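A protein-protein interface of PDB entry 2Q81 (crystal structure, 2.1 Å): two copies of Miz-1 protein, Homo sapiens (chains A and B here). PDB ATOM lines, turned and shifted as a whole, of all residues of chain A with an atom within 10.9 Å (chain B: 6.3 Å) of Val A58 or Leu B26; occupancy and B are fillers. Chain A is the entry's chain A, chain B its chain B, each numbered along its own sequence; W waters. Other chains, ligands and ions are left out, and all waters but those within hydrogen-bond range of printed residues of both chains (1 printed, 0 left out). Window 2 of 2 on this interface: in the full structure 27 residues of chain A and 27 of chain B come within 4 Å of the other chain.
OE1 of Gln B21 lies close to O of Ala A44, at 3.0 Å.
The backbone carbonyl oxygen (O) of Phe A57 sits at hydrogen-bond distance from the side-chain amide nitrogen (NE2) of Gln A60.
The side-chain amide nitrogen (NE2) of Gln B21 is in hydrogen-bond range of a ring nitrogen (NE2) of His B42 (2.9 Å).
O of Val A58 sits close to OE1 of Gln A60.
The side-chain carboxylate (OD1) of Asp A29 lies within salt-bridge range of the side-chain amino group (NZ) of Lys A43 (2.9 Å).
N of Leu B26 is in hydrogen-bond range of O of Gln B21 (2.8 Å).
The side-chain sulfur of Cys B28 lies within hydrogen-bond range of the backbone carbonyl oxygen of Leu B26, at 3.5 Å.
Among the printed residues, pairs that only touch across the chains: Lys A43 with Leu B27, Ala A44 with Leu B18, Ala A44 with Leu B27, Ala A44 with His B42, Ala A47 with Gln B21, Ala A47 with Leu B27, Ala A48 with Gln B21, Phe A57 with Leu B27 and Val A58 with Leu B26.
Printed residues of chain B within 4 Å of Val A58: Leu B26 (3.95 Å).
Leu B26 touches just one residue of chain A: Val A58 (3.95 Å).
Gln B21 touches just these residues of chain A: Ala A44, Ala A47 and Ala A48.
No residue of chain A comes within 4 Å of Leu B24.
No residue of chain A comes within 4 Å of Gly B25.
No residue of chain A comes within 4 Å of Cys B28.
Of the printed residues of chain B, Ala A44 touches Leu B18 (3.6 Å), Gln B21 (3.0 Å), Leu B27 (3.9 Å) and His B42 (3.4 Å).
Of the printed residues of chain A, His B42 touches Ala A44.
Of the printed residues of chain B, Ala A48 touches Gln B21 (3.8 Å).
Of the printed residues of chain B, Ala A47 touches Gln B21 (3.8 Å) and Leu B27 (3.4 Å).
Of the 12 printed residues of chain B, 5 touch a printed residue of chain A.
Hydrophobic or aromatic side chains of chain B that line the printed part of chain A: Leu B18, Leu B26, Leu B27 and His B42.
Of the 24 printed residues of chain A, 6 touch a printed residue of chain B.
Printed residues of chain A that touch a printed residue of chain B: Lys A43, Ala A44, Ala A47, Ala A48, Phe A57 and Val A58.
Hydrophobic or aromatic side chains of chain A within 4 Å of the printed part of chain B: Ala A44, Ala A47, Phe A57 and Val A58.
1 position is printed for both chains.
Of the 10 pairs that touch across the chains among the printed residues, none has its exchanged pair printed and touching as well.
Water W1 bridges the side-chain amide oxygen (OE1) of Gln B21 (3.1 Å) and the backbone carbonyl oxygen (O) of Ala A47 (3.4 Å).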
ATOM      1  N   ASP A  29     -20.061  15.119  23.667  1.00  0.00           N
ATOM      2  CA  ASP A  29     -19.106  14.588  24.645  1.00  0.00           C
ATOM      3  C   ASP A  29     -19.581  14.713  26.098  1.00  0.00           C
ATOM      4  O   ASP A  29     -18.904  14.275  27.026  1.00  0.00           O
ATOM      5  CB  ASP A  29     -17.746  15.271  24.435  1.00  0.00           C
ATOM      6  CG  ASP A  29     -17.876  16.774  24.422  1.00  0.00           C
ATOM      7  OD1 ASP A  29     -18.056  17.324  25.490  1.00  0.00           O
ATOM      8  OD2 ASP A  29     -17.860  17.394  23.346  1.00  0.00           O
ATOM      9  N   CYS A  30     -20.751  15.309  26.297  1.00  0.00           N
ATOM     10  CA  CYS A  30     -21.358  15.397  27.634  1.00  0.00           C
ATOM     11  C   CYS A  30     -22.861  15.158  27.583  1.00  0.00           C
ATOM     12  O   CYS A  30     -23.546  15.659  26.666  1.00  0.00           O
ATOM     13  CB  CYS A  30     -21.065  16.750  28.305  1.00  0.00           C
ATOM     14  SG  CYS A  30     -21.490  16.841  30.107  1.00  0.00           S
ATOM     15  N   HIS A  42     -21.717  19.521  23.827  1.00  0.00           N
ATOM     16  CA  HIS A  42     -20.261  19.594  23.725  1.00  0.00           C
ATOM     17  C   HIS A  42     -19.819  20.454  24.871  1.00  0.00           C
ATOM     18  O   HIS A  42     -20.275  21.585  24.961  1.00  0.00           O
ATOM     19  CB  HIS A  42     -19.826  20.293  22.402  1.00  0.00           C
ATOM     20  CG  HIS A  42     -20.343  19.630  21.156  1.00  0.00           C
ATOM     21  ND1 HIS A  42     -21.572  19.929  20.608  1.00  0.00           N
ATOM     22  CD2 HIS A  42     -19.774  18.722  20.327  1.00  0.00           C
ATOM     23  CE1 HIS A  42     -21.751  19.217  19.505  1.00  0.00           C
ATOM     24  NE2 HIS A  42     -20.684  18.453  19.324  1.00  0.00           N
ATOM     25  N   LYS A  43     -18.912  19.962  25.724  1.00  0.00           N
ATOM     26  CA  LYS A  43     -18.380  20.782  26.816  1.00  0.00           C
ATOM     27  C   LYS A  43     -17.735  22.071  26.296  1.00  0.00           C
ATOM     28  O   LYS A  43     -17.886  23.122  26.909  1.00  0.00           O
ATOM     29  CB  LYS A  43     -17.348  20.023  27.661  1.00  0.00           C
ATOM     30  CG  LYS A  43     -17.918  18.842  28.487  1.00  0.00           C
ATOM     31  CD  LYS A  43     -16.809  18.224  29.330  1.00  0.00           C
ATOM     32  CE  LYS A  43     -15.722  17.581  28.479  1.00  0.00           C
ATOM     33  NZ  LYS A  43     -16.271  16.449  27.661  1.00  0.00           N
ATOM     34  N   ALA A  44     -17.024  21.988  25.165  1.00  0.00           N
ATOM     35  CA  ALA A  44     -16.346  23.168  24.586  1.00  0.00           C
ATOM     36  C   ALA A  44     -17.302  24.309  24.239  1.00  0.00           C
ATOM     37  O   ALA A  44     -16.996  25.492  24.463  1.00  0.00           O
ATOM     38  CB  ALA A  44     -15.519  22.763  23.347  1.00  0.00           C
ATOM     39  N   VAL A  45     -18.451  23.965  23.669  1.00  0.00           N
ATOM     40  CA  VAL A  45     -19.479  24.967  23.336  1.00  0.00           C
ATOM     41  C   VAL A  45     -20.106  25.571  24.591  1.00  0.00           C
ATOM     42  O   VAL A  45     -20.359  26.785  24.653  1.00  0.00           O
ATOM     43  CB  VAL A  45     -20.588  24.365  22.465  1.00  0.00           C
ATOM     44  CG1 VAL A  45     -21.771  25.351  22.336  1.00  0.00           C
ATOM     45  CG2 VAL A  45     -20.039  23.935  21.083  1.00  0.00           C
ATOM     46  N   LEU A  46     -20.349  24.732  25.593  1.00  0.00           N
ATOM     47  CA  LEU A  46     -20.937  25.193  26.851  1.00  0.00           C
ATOM     48  C   LEU A  46     -19.997  26.155  27.576  1.00  0.00           C
ATOM     49  O   LEU A  46     -20.437  27.195  28.116  1.00  0.00           O
ATOM     50  CB  LEU A  46     -21.344  24.002  27.740  1.00  0.00           C
ATOM     51  CG  LEU A  46     -22.760  23.393  27.569  1.00  0.00           C
ATOM     52  CD1 LEU A  46     -23.097  22.978  26.151  1.00  0.00           C
ATOM     53  CD2 LEU A  46     -22.893  22.157  28.451  1.00  0.00           C
ATOM     54  N   ALA A  47     -18.706  25.820  27.576  1.00  0.00           N
ATOM     55  CA  ALA A  47     -17.668  26.681  28.147  1.00  0.00           C
ATOM     56  C   ALA A  47     -17.462  27.961  27.315  1.00  0.00           C
ATOM     57  O   ALA A  47     -17.109  29.002  27.854  1.00  0.00           O
ATOM     58  CB  ALA A  47     -16.360  25.919  28.282  1.00  0.00           C
ATOM     59  N   ALA A  48     -17.684  27.878  26.005  1.00  0.00           N
ATOM     60  CA  ALA A  48     -17.603  29.067  25.143  1.00  0.00           C
ATOM     61  C   ALA A  48     -18.700  30.083  25.471  1.00  0.00           C
ATOM     62  O   ALA A  48     -18.510  31.286  25.286  1.00  0.00           O
ATOM     63  CB  ALA A  48     -17.697  28.672  23.661  1.00  0.00           C
ATOM     64  N   CYS A  49     -19.834  29.590  25.968  1.00  0.00           N
ATOM     65  CA  CYS A  49     -21.049  30.400  26.124  1.00  0.00           C
ATOM     66  C   CYS A  49     -21.460  30.675  27.571  1.00  0.00           C
ATOM     67  O   CYS A  49     -22.416  31.415  27.817  1.00  0.00           O
ATOM     68  CB  CYS A  49     -22.213  29.736  25.385  1.00  0.00           C
ATOM     69  SG  CYS A  49     -22.173  30.013  23.592  1.00  0.00           S
ATOM     70  N   SER A  50     -20.749  30.068  28.516  1.00  0.00           N
ATOM     71  CA  SER A  50     -21.038  30.250  29.944  1.00  0.00           C
ATOM     72  C   SER A  50     -19.768  30.182  30.793  1.00  0.00           C
ATOM     73  O   SER A  50     -19.037  29.189  30.744  1.00  0.00           O
ATOM     74  CB  SER A  50     -22.025  29.154  30.400  1.00  0.00           C
ATOM     75  OG  SER A  50     -22.143  29.136  31.813  1.00  0.00           O
ATOM     76  N   GLU A  51     -19.520  31.224  31.584  1.00  0.00           N
ATOM     77  CA  GLU A  51     -18.400  31.246  32.519  1.00  0.00           C
ATOM     78  C   GLU A  51     -18.508  30.164  33.583  1.00  0.00           C
ATOM     79  O   GLU A  51     -17.493  29.592  33.983  1.00  0.00           O
ATOM     80  CB  GLU A  51     -18.239  32.627  33.192  1.00  0.00           C
ATOM     81  CG  GLU A  51     -17.314  33.577  32.441  1.00  0.00           C
ATOM     82  CD  GLU A  51     -15.907  33.002  32.213  1.00  0.00           C
ATOM     83  OE1 GLU A  51     -15.136  32.851  33.196  1.00  0.00           O
ATOM     84  OE2 GLU A  51     -15.580  32.711  31.039  1.00  0.00           O
ATOM     85  N   TYR A  52     -19.723  29.899  34.050  1.00  0.00           N
ATOM     86  CA  TYR A  52     -19.949  28.768  34.960  1.00  0.00           C
ATOM     87  C   TYR A  52     -19.456  27.438  34.365  1.00  0.00           C
ATOM     88  O   TYR A  52     -18.729  26.686  35.000  1.00  0.00           O
ATOM     89  CB  TYR A  52     -21.425  28.612  35.340  1.00  0.00           C
ATOM     90  CG  TYR A  52     -21.605  27.393  36.213  1.00  0.00           C
ATOM     91  CD1 TYR A  52     -21.391  27.464  37.599  1.00  0.00           C
ATOM     92  CD2 TYR A  52     -21.906  26.151  35.655  1.00  0.00           C
ATOM     93  CE1 TYR A  52     -21.519  26.329  38.394  1.00  0.00           C
ATOM     94  CE2 TYR A  52     -22.036  25.010  36.444  1.00  0.00           C
ATOM     95  CZ  TYR A  52     -21.844  25.106  37.798  1.00  0.00           C
ATOM     96  OH  TYR A  52     -21.973  23.970  38.562  1.00  0.00           O
ATOM     97  N   PHE A  53     -19.877  27.147  33.145  1.00  0.00           N
ATOM     98  CA  PHE A  53     -19.501  25.889  32.517  1.00  0.00           C
ATOM     99  C   PHE A  53     -18.002  25.832  32.238  1.00  0.00           C
ATOM    100  O   PHE A  53     -17.373  24.790  32.420  1.00  0.00           O
ATOM    101  CB  PHE A  53     -20.321  25.655  31.255  1.00  0.00           C
ATOM    102  CG  PHE A  53     -21.681  25.022  31.519  1.00  0.00           C
ATOM    103  CD1 PHE A  53     -21.822  24.021  32.475  1.00  0.00           C
ATOM    104  CD2 PHE A  53     -22.800  25.404  30.791  1.00  0.00           C
ATOM    105  CE1 PHE A  53     -23.074  23.419  32.718  1.00  0.00           C
ATOM    106  CE2 PHE A  53     -24.058  24.782  31.013  1.00  0.00           C
ATOM    107  CZ  PHE A  53     -24.182  23.801  31.984  1.00  0.00           C
ATOM    108  N   LYS A  54     -17.438  26.961  31.824  1.00  0.00           N
ATOM    109  CA  LYS A  54     -15.993  27.095  31.637  1.00  0.00           C
ATOM    110  C   LYS A  54     -15.235  26.671  32.908  1.00  0.00           C
ATOM    111  O   LYS A  54     -14.385  25.787  32.857  1.00  0.00           O
ATOM    112  CB  LYS A  54     -15.656  28.533  31.223  1.00  0.00           C
ATOM    113  CG  LYS A  54     -14.174  28.829  30.857  1.00  0.00           C
ATOM    114  CD  LYS A  54     -14.109  30.145  30.076  1.00  0.00           C
ATOM    115  CE  LYS A  54     -12.704  30.684  29.873  1.00  0.00           C
ATOM    116  NZ  LYS A  54     -12.750  32.186  29.756  1.00  0.00           N
ATOM    117  N   MET A  55     -15.570  27.277  34.041  1.00  0.00           N
ATOM    118  CA  MET A  55     -14.871  26.991  35.301  1.00  0.00           C
ATOM    119  C   MET A  55     -15.232  25.622  35.901  1.00  0.00           C
ATOM    120  O   MET A  55     -14.451  25.053  36.665  1.00  0.00           O
ATOM    121  CB  MET A  55     -15.101  28.113  36.320  1.00  0.00           C
ATOM    122  CG  MET A  55     -14.575  29.484  35.869  1.00  0.00           C
ATOM    123  SD  MET A  55     -14.732  30.778  37.126  1.00  0.00           S
ATOM    124  CE  MET A  55     -16.527  30.882  37.210  1.00  0.00           C
ATOM    125  N   LEU A  56     -16.416  25.109  35.574  1.00  0.00           N
ATOM    126  CA  LEU A  56     -16.787  23.751  35.962  1.00  0.00           C
ATOM    127  C   LEU A  56     -15.942  22.711  35.213  1.00  0.00           C
ATOM    128  O   LEU A  56     -15.324  21.850  35.832  1.00  0.00           O
ATOM    129  CB  LEU A  56     -18.272  23.471  35.676  1.00  0.00           C
ATOM    130  CG  LEU A  56     -18.698  22.005  35.878  1.00  0.00           C
ATOM    131  CD1 LEU A  56     -18.599  21.617  37.352  1.00  0.00           C
ATOM    132  CD2 LEU A  56     -20.101  21.716  35.355  1.00  0.00           C
ATOM    133  N   PHE A  57     -15.945  22.787  33.883  1.00  0.00           N
ATOM    134  CA  PHE A  57     -15.324  21.749  33.056  1.00  0.00           C
ATOM    135  C   PHE A  57     -13.799  21.866  33.046  1.00  0.00           C
ATOM    136  O   PHE A  57     -13.110  20.853  33.010  1.00  0.00           O
ATOM    137  CB  PHE A  57     -15.871  21.763  31.620  1.00  0.00           C
ATOM    138  CG  PHE A  57     -17.321  21.334  31.500  1.00  0.00           C
ATOM    139  CD1 PHE A  57     -17.789  20.179  32.141  1.00  0.00           C
ATOM    140  CD2 PHE A  57     -18.207  22.064  30.704  1.00  0.00           C
ATOM    141  CE1 PHE A  57     -19.132  19.784  32.017  1.00  0.00           C
ATOM    142  CE2 PHE A  57     -19.553  21.677  30.577  1.00  0.00           C
ATOM    143  CZ  PHE A  57     -20.012  20.527  31.226  1.00  0.00           C
ATOM    144  N   VAL A  58     -13.290  23.096  33.078  1.00  0.00           N
ATOM    145  CA  VAL A  58     -11.837  23.341  33.121  1.00  0.00           C
ATOM    146  C   VAL A  58     -11.277  23.241  34.544  1.00  0.00           C
ATOM    147  O   VAL A  58     -10.294  22.526  34.780  1.00  0.00           O
ATOM    148  CB  VAL A  58     -11.453  24.713  32.498  1.00  0.00           C
ATOM    149  CG1 VAL A  58      -9.934  24.961  32.576  1.00  0.00           C
ATOM    150  CG2 VAL A  58     -11.944  24.811  31.043  1.00  0.00           C
ATOM    151  N   ASP A  59     -11.907  23.954  35.483  1.00  0.00           N
ATOM    152  CA  ASP A  59     -11.371  24.120  36.833  1.00  0.00           C
ATOM    153  C   ASP A  59     -12.060  23.277  37.914  1.00  0.00           C
ATOM    154  O   ASP A  59     -11.664  23.340  39.072  1.00  0.00           O
ATOM    155  CB  ASP A  59     -11.402  25.603  37.229  1.00  0.00           C
ATOM    156  CG  ASP A  59     -10.604  26.478  36.269  1.00  0.00           C
ATOM    157  OD1 ASP A  59      -9.378  26.255  36.158  1.00  0.00           O
ATOM    158  OD2 ASP A  59     -11.201  27.381  35.623  1.00  0.00           O
ATOM    159  N   GLN A  60     -13.078  22.495  37.539  1.00  0.00           N
ATOM    160  CA  GLN A  60     -13.810  21.625  38.491  1.00  0.00           C
ATOM    161  C   GLN A  60     -14.466  22.395  39.650  1.00  0.00           C
ATOM    162  O   GLN A  60     -14.506  21.919  40.782  1.00  0.00           O
ATOM    163  CB  GLN A  60     -12.904  20.501  39.029  1.00  0.00           C
ATOM    164  CG  GLN A  60     -12.785  19.294  38.098  1.00  0.00           C
ATOM    165  CD  GLN A  60     -11.965  19.571  36.841  1.00  0.00           C
ATOM    166  OE1 GLN A  60     -10.824  20.062  36.913  1.00  0.00           O
ATOM    167  NE2 GLN A  60     -12.535  19.243  35.681  1.00  0.00           N
ATOM    168  N   LYS A  61     -15.003  23.568  39.338  1.00  0.00           N
ATOM    169  CA  LYS A  61     -15.455  24.531  40.341  1.00  0.00           C
ATOM    170  C   LYS A  61     -16.986  24.614  40.459  1.00  0.00           C
ATOM    171  O   LYS A  61     -17.692  24.596  39.437  1.00  0.00           O
ATOM    172  CB  LYS A  61     -14.843  25.902  39.995  1.00  0.00           C
ATOM    173  CG  LYS A  61     -15.612  27.126  40.447  1.00  0.00           C
ATOM    174  CD  LYS A  61     -14.759  28.380  40.297  1.00  0.00           C
ATOM    175  CE  LYS A  61     -15.091  29.415  41.370  1.00  0.00           C
ATOM    176  NZ  LYS A  61     -16.493  29.917  41.233  1.00  0.00           N
ATOM    177  N   ASP A  62     -17.473  24.698  41.705  1.00  0.00           N
ATOM    178  CA  ASP A  62     -18.886  24.992  42.016  1.00  0.00           C
ATOM    179  C   ASP A  62     -19.845  23.947  41.390  1.00  0.00           C
ATOM    180  O   ASP A  62     -20.911  24.276  40.850  1.00  0.00           O
ATOM    181  CB  ASP A  62     -19.219  26.414  41.545  1.00  0.00           C
ATOM    182  CG  ASP A  62     -20.191  27.142  42.454  1.00  0.00           C
ATOM    183  OD1 ASP A  62     -20.006  27.132  43.691  1.00  0.00           O
ATOM    184  OD2 ASP A  62     -21.129  27.778  41.914  1.00  0.00           O
ATOM    185  N   VAL A  63     -19.442  22.686  41.484  1.00  0.00           N
ATOM    186  CA  VAL A  63     -20.149  21.565  40.849  1.00  0.00           C
ATOM    187  C   VAL A  63     -21.582  21.424  41.357  1.00  0.00           C
ATOM    188  O   VAL A  63     -22.494  21.190  40.578  1.00  0.00           O
ATOM    189  CB  VAL A  63     -19.418  20.221  41.114  1.00  0.00           C
ATOM    190  CG1 VAL A  63     -19.841  19.174  40.101  1.00  0.00           C
ATOM    191  CG2 VAL A  63     -17.883  20.417  41.110  1.00  0.00           C
ATOM    192  N   LEU B  18     -13.537  28.813  21.019  1.00  0.00           N
ATOM    193  CA  LEU B  18     -13.007  27.496  20.629  1.00  0.00           C
ATOM    194  C   LEU B  18     -11.530  27.562  20.220  1.00  0.00           C
ATOM    195  O   LEU B  18     -10.743  26.686  20.577  1.00  0.00           O
ATOM    196  CB  LEU B  18     -13.848  26.878  19.501  1.00  0.00           C
ATOM    197  CG  LEU B  18     -15.284  26.488  19.892  1.00  0.00           C
ATOM    198  CD1 LEU B  18     -16.117  25.982  18.698  1.00  0.00           C
ATOM    199  CD2 LEU B  18     -15.283  25.450  20.996  1.00  0.00           C
ATOM    200  N   GLN B  20      -9.439  29.946  21.230  1.00  0.00           N
ATOM    201  CA  GLN B  20      -8.763  30.221  22.495  1.00  0.00           C
ATOM    202  C   GLN B  20      -8.506  28.921  23.261  1.00  0.00           C
ATOM    203  O   GLN B  20      -7.378  28.659  23.670  1.00  0.00           O
ATOM    204  CB  GLN B  20      -9.560  31.213  23.345  1.00  0.00           C
ATOM    205  CG  GLN B  20      -8.881  31.623  24.642  1.00  0.00           C
ATOM    206  CD  GLN B  20      -9.736  32.567  25.472  1.00  0.00           C
ATOM    207  OE1 GLN B  20     -10.523  32.123  26.301  1.00  0.00           O
ATOM    208  NE2 GLN B  20      -9.595  33.863  25.246  1.00  0.00           N
ATOM    209  N   GLN B  21      -9.556  28.121  23.428  1.00  0.00           N
ATOM    210  CA  GLN B  21      -9.467  26.805  24.067  1.00  0.00           C
ATOM    211  C   GLN B  21      -8.378  25.903  23.461  1.00  0.00           C
ATOM    212  O   GLN B  21      -7.579  25.323  24.190  1.00  0.00           O
ATOM    213  CB  GLN B  21     -10.809  26.087  23.983  1.00  0.00           C
ATOM    214  CG  GLN B  21     -11.859  26.609  24.979  1.00  0.00           C
ATOM    215  CD  GLN B  21     -13.242  26.017  24.735  1.00  0.00           C
ATOM    216  OE1 GLN B  21     -14.271  26.587  25.125  1.00  0.00           O
ATOM    217  NE2 GLN B  21     -13.270  24.878  24.109  1.00  0.00           N
ATOM    218  N   ARG B  22      -8.348  25.786  22.139  1.00  0.00           N
ATOM    219  CA  ARG B  22      -7.469  24.797  21.535  1.00  0.00           C
ATOM    220  C   ARG B  22      -6.012  25.247  21.602  1.00  0.00           C
ATOM    221  O   ARG B  22      -5.114  24.435  21.774  1.00  0.00           O
ATOM    222  CB  ARG B  22      -7.944  24.399  20.131  1.00  0.00           C
ATOM    223  CG  ARG B  22      -7.886  25.470  19.076  1.00  0.00           C
ATOM    224  CD  ARG B  22      -6.809  25.153  18.023  1.00  0.00           C
ATOM    225  NE  ARG B  22      -6.658  26.280  17.099  1.00  0.00           N
ATOM    226  CZ  ARG B  22      -5.666  26.414  16.218  1.00  0.00           C
ATOM    227  NH1 ARG B  22      -5.606  27.496  15.447  1.00  0.00           N
ATOM    228  NH2 ARG B  22      -4.739  25.474  16.110  1.00  0.00           N
ATOM    229  N   GLN B  23      -5.820  26.558  21.578  1.00  0.00           N
ATOM    230  CA  GLN B  23      -4.534  27.177  21.765  1.00  0.00           C
ATOM    231  C   GLN B  23      -3.990  26.855  23.166  1.00  0.00           C
ATOM    232  O   GLN B  23      -2.786  26.694  23.361  1.00  0.00           O
ATOM    233  CB  GLN B  23      -4.704  28.688  21.610  1.00  0.00           C
ATOM    234  CG  GLN B  23      -3.588  29.347  20.899  1.00  0.00           C
ATOM    235  CD  GLN B  23      -3.678  29.155  19.410  1.00  0.00           C
ATOM    236  OE1 GLN B  23      -2.668  29.047  18.736  1.00  0.00           O
ATOM    237  NE2 GLN B  23      -4.889  29.119  18.891  1.00  0.00           N
ATOM    238  N   LEU B  24      -4.900  26.765  24.130  1.00  0.00           N
ATOM    239  CA  LEU B  24      -4.545  26.484  25.509  1.00  0.00           C
ATOM    240  C   LEU B  24      -4.644  24.994  25.832  1.00  0.00           C
ATOM    241  O   LEU B  24      -4.272  24.579  26.927  1.00  0.00           O
ATOM    242  CB  LEU B  24      -5.447  27.283  26.452  1.00  0.00           C
ATOM    243  CG  LEU B  24      -5.356  28.809  26.371  1.00  0.00           C
ATOM    244  CD1 LEU B  24      -6.418  29.439  27.270  1.00  0.00           C
ATOM    245  CD2 LEU B  24      -3.959  29.272  26.764  1.00  0.00           C
ATOM    246  N   GLY B  25      -5.156  24.204  24.886  1.00  0.00           N
ATOM    247  CA  GLY B  25      -5.372  22.773  25.098  1.00  0.00           C
ATOM    248  C   GLY B  25      -6.483  22.500  26.102  1.00  0.00           C
ATOM    249  O   GLY B  25      -6.463  21.486  26.818  1.00  0.00           O
ATOM    250  N   LEU B  26      -7.450  23.411  26.169  1.00  0.00           N
ATOM    251  CA  LEU B  26      -8.571  23.275  27.089  1.00  0.00           C
ATOM    252  C   LEU B  26      -9.721  22.553  26.403  1.00  0.00           C
ATOM    253  O   LEU B  26     -10.078  22.879  25.279  1.00  0.00           O
ATOM    254  CB  LEU B  26      -9.028  24.655  27.586  1.00  0.00           C
ATOM    255  CG  LEU B  26      -7.989  25.470  28.365  1.00  0.00           C
ATOM    256  CD1 LEU B  26      -8.596  26.798  28.837  1.00  0.00           C
ATOM    257  CD2 LEU B  26      -7.423  24.660  29.537  1.00  0.00           C
ATOM    258  N   LEU B  27     -10.293  21.572  27.093  1.00  0.00           N
ATOM    259  CA  LEU B  27     -11.477  20.852  26.609  1.00  0.00           C
ATOM    260  C   LEU B  27     -11.267  20.192  25.249  1.00  0.00           C
ATOM    261  O   LEU B  27     -12.221  19.995  24.487  1.00  0.00           O
ATOM    262  CB  LEU B  27     -12.710  21.774  26.587  1.00  0.00           C
ATOM    263  CG  LEU B  27     -12.951  22.503  27.919  1.00  0.00           C
ATOM    264  CD1 LEU B  27     -14.176  23.363  27.823  1.00  0.00           C
ATOM    265  CD2 LEU B  27     -13.118  21.478  29.057  1.00  0.00           C
ATOM    266  N   CYS B  28     -10.028  19.848  24.950  1.00  0.00           N
ATOM    267  CA  CYS B  28      -9.731  19.248  23.655  1.00  0.00           C
ATOM    268  C   CYS B  28      -9.727  17.729  23.818  1.00  0.00           C
ATOM    269  O   CYS B  28      -9.302  17.209  24.862  1.00  0.00           O
ATOM    270  CB  CYS B  28      -8.397  19.755  23.127  1.00  0.00           C
ATOM    271  SG  CYS B  28      -8.485  21.473  22.525  1.00  0.00           S
ATOM    272  N   LYS B  40      -3.412  20.280  19.738  1.00  0.00           N
ATOM    273  CA  LYS B  40      -4.680  19.894  20.324  1.00  0.00           C
ATOM    274  C   LYS B  40      -5.829  20.500  19.546  1.00  0.00           C
ATOM    275  O   LYS B  40      -5.693  21.564  18.952  1.00  0.00           O
ATOM    276  CB  LYS B  40      -4.717  20.274  21.804  1.00  0.00           C
ATOM    277  CG  LYS B  40      -4.221  19.131  22.698  1.00  0.00           C
ATOM    278  CD  LYS B  40      -3.414  19.631  23.867  1.00  0.00           C
ATOM    279  CE  LYS B  40      -3.607  18.726  25.091  1.00  0.00           C
ATOM    280  NZ  LYS B  40      -3.032  17.357  24.935  1.00  0.00           N
ATOM    281  N   HIS B  42     -10.545  20.078  18.942  1.00  0.00           N
ATOM    282  CA  HIS B  42     -11.818  19.461  19.297  1.00  0.00           C
ATOM    283  C   HIS B  42     -12.255  18.577  18.111  1.00  0.00           C
ATOM    284  O   HIS B  42     -12.356  19.076  16.980  1.00  0.00           O
ATOM    285  CB  HIS B  42     -12.903  20.527  19.555  1.00  0.00           C
ATOM    286  CG  HIS B  42     -12.501  21.621  20.517  1.00  0.00           C
ATOM    287  ND1 HIS B  42     -11.842  22.765  20.114  1.00  0.00           N
ATOM    288  CD2 HIS B  42     -12.684  21.750  21.852  1.00  0.00           C
ATOM    289  CE1 HIS B  42     -11.653  23.560  21.153  1.00  0.00           C
ATOM    290  NE2 HIS B  42     -12.154  22.966  22.222  1.00  0.00           N
HETATM  291  O   HOH W   1     -14.053  29.440  26.396  1.00  0.00           O
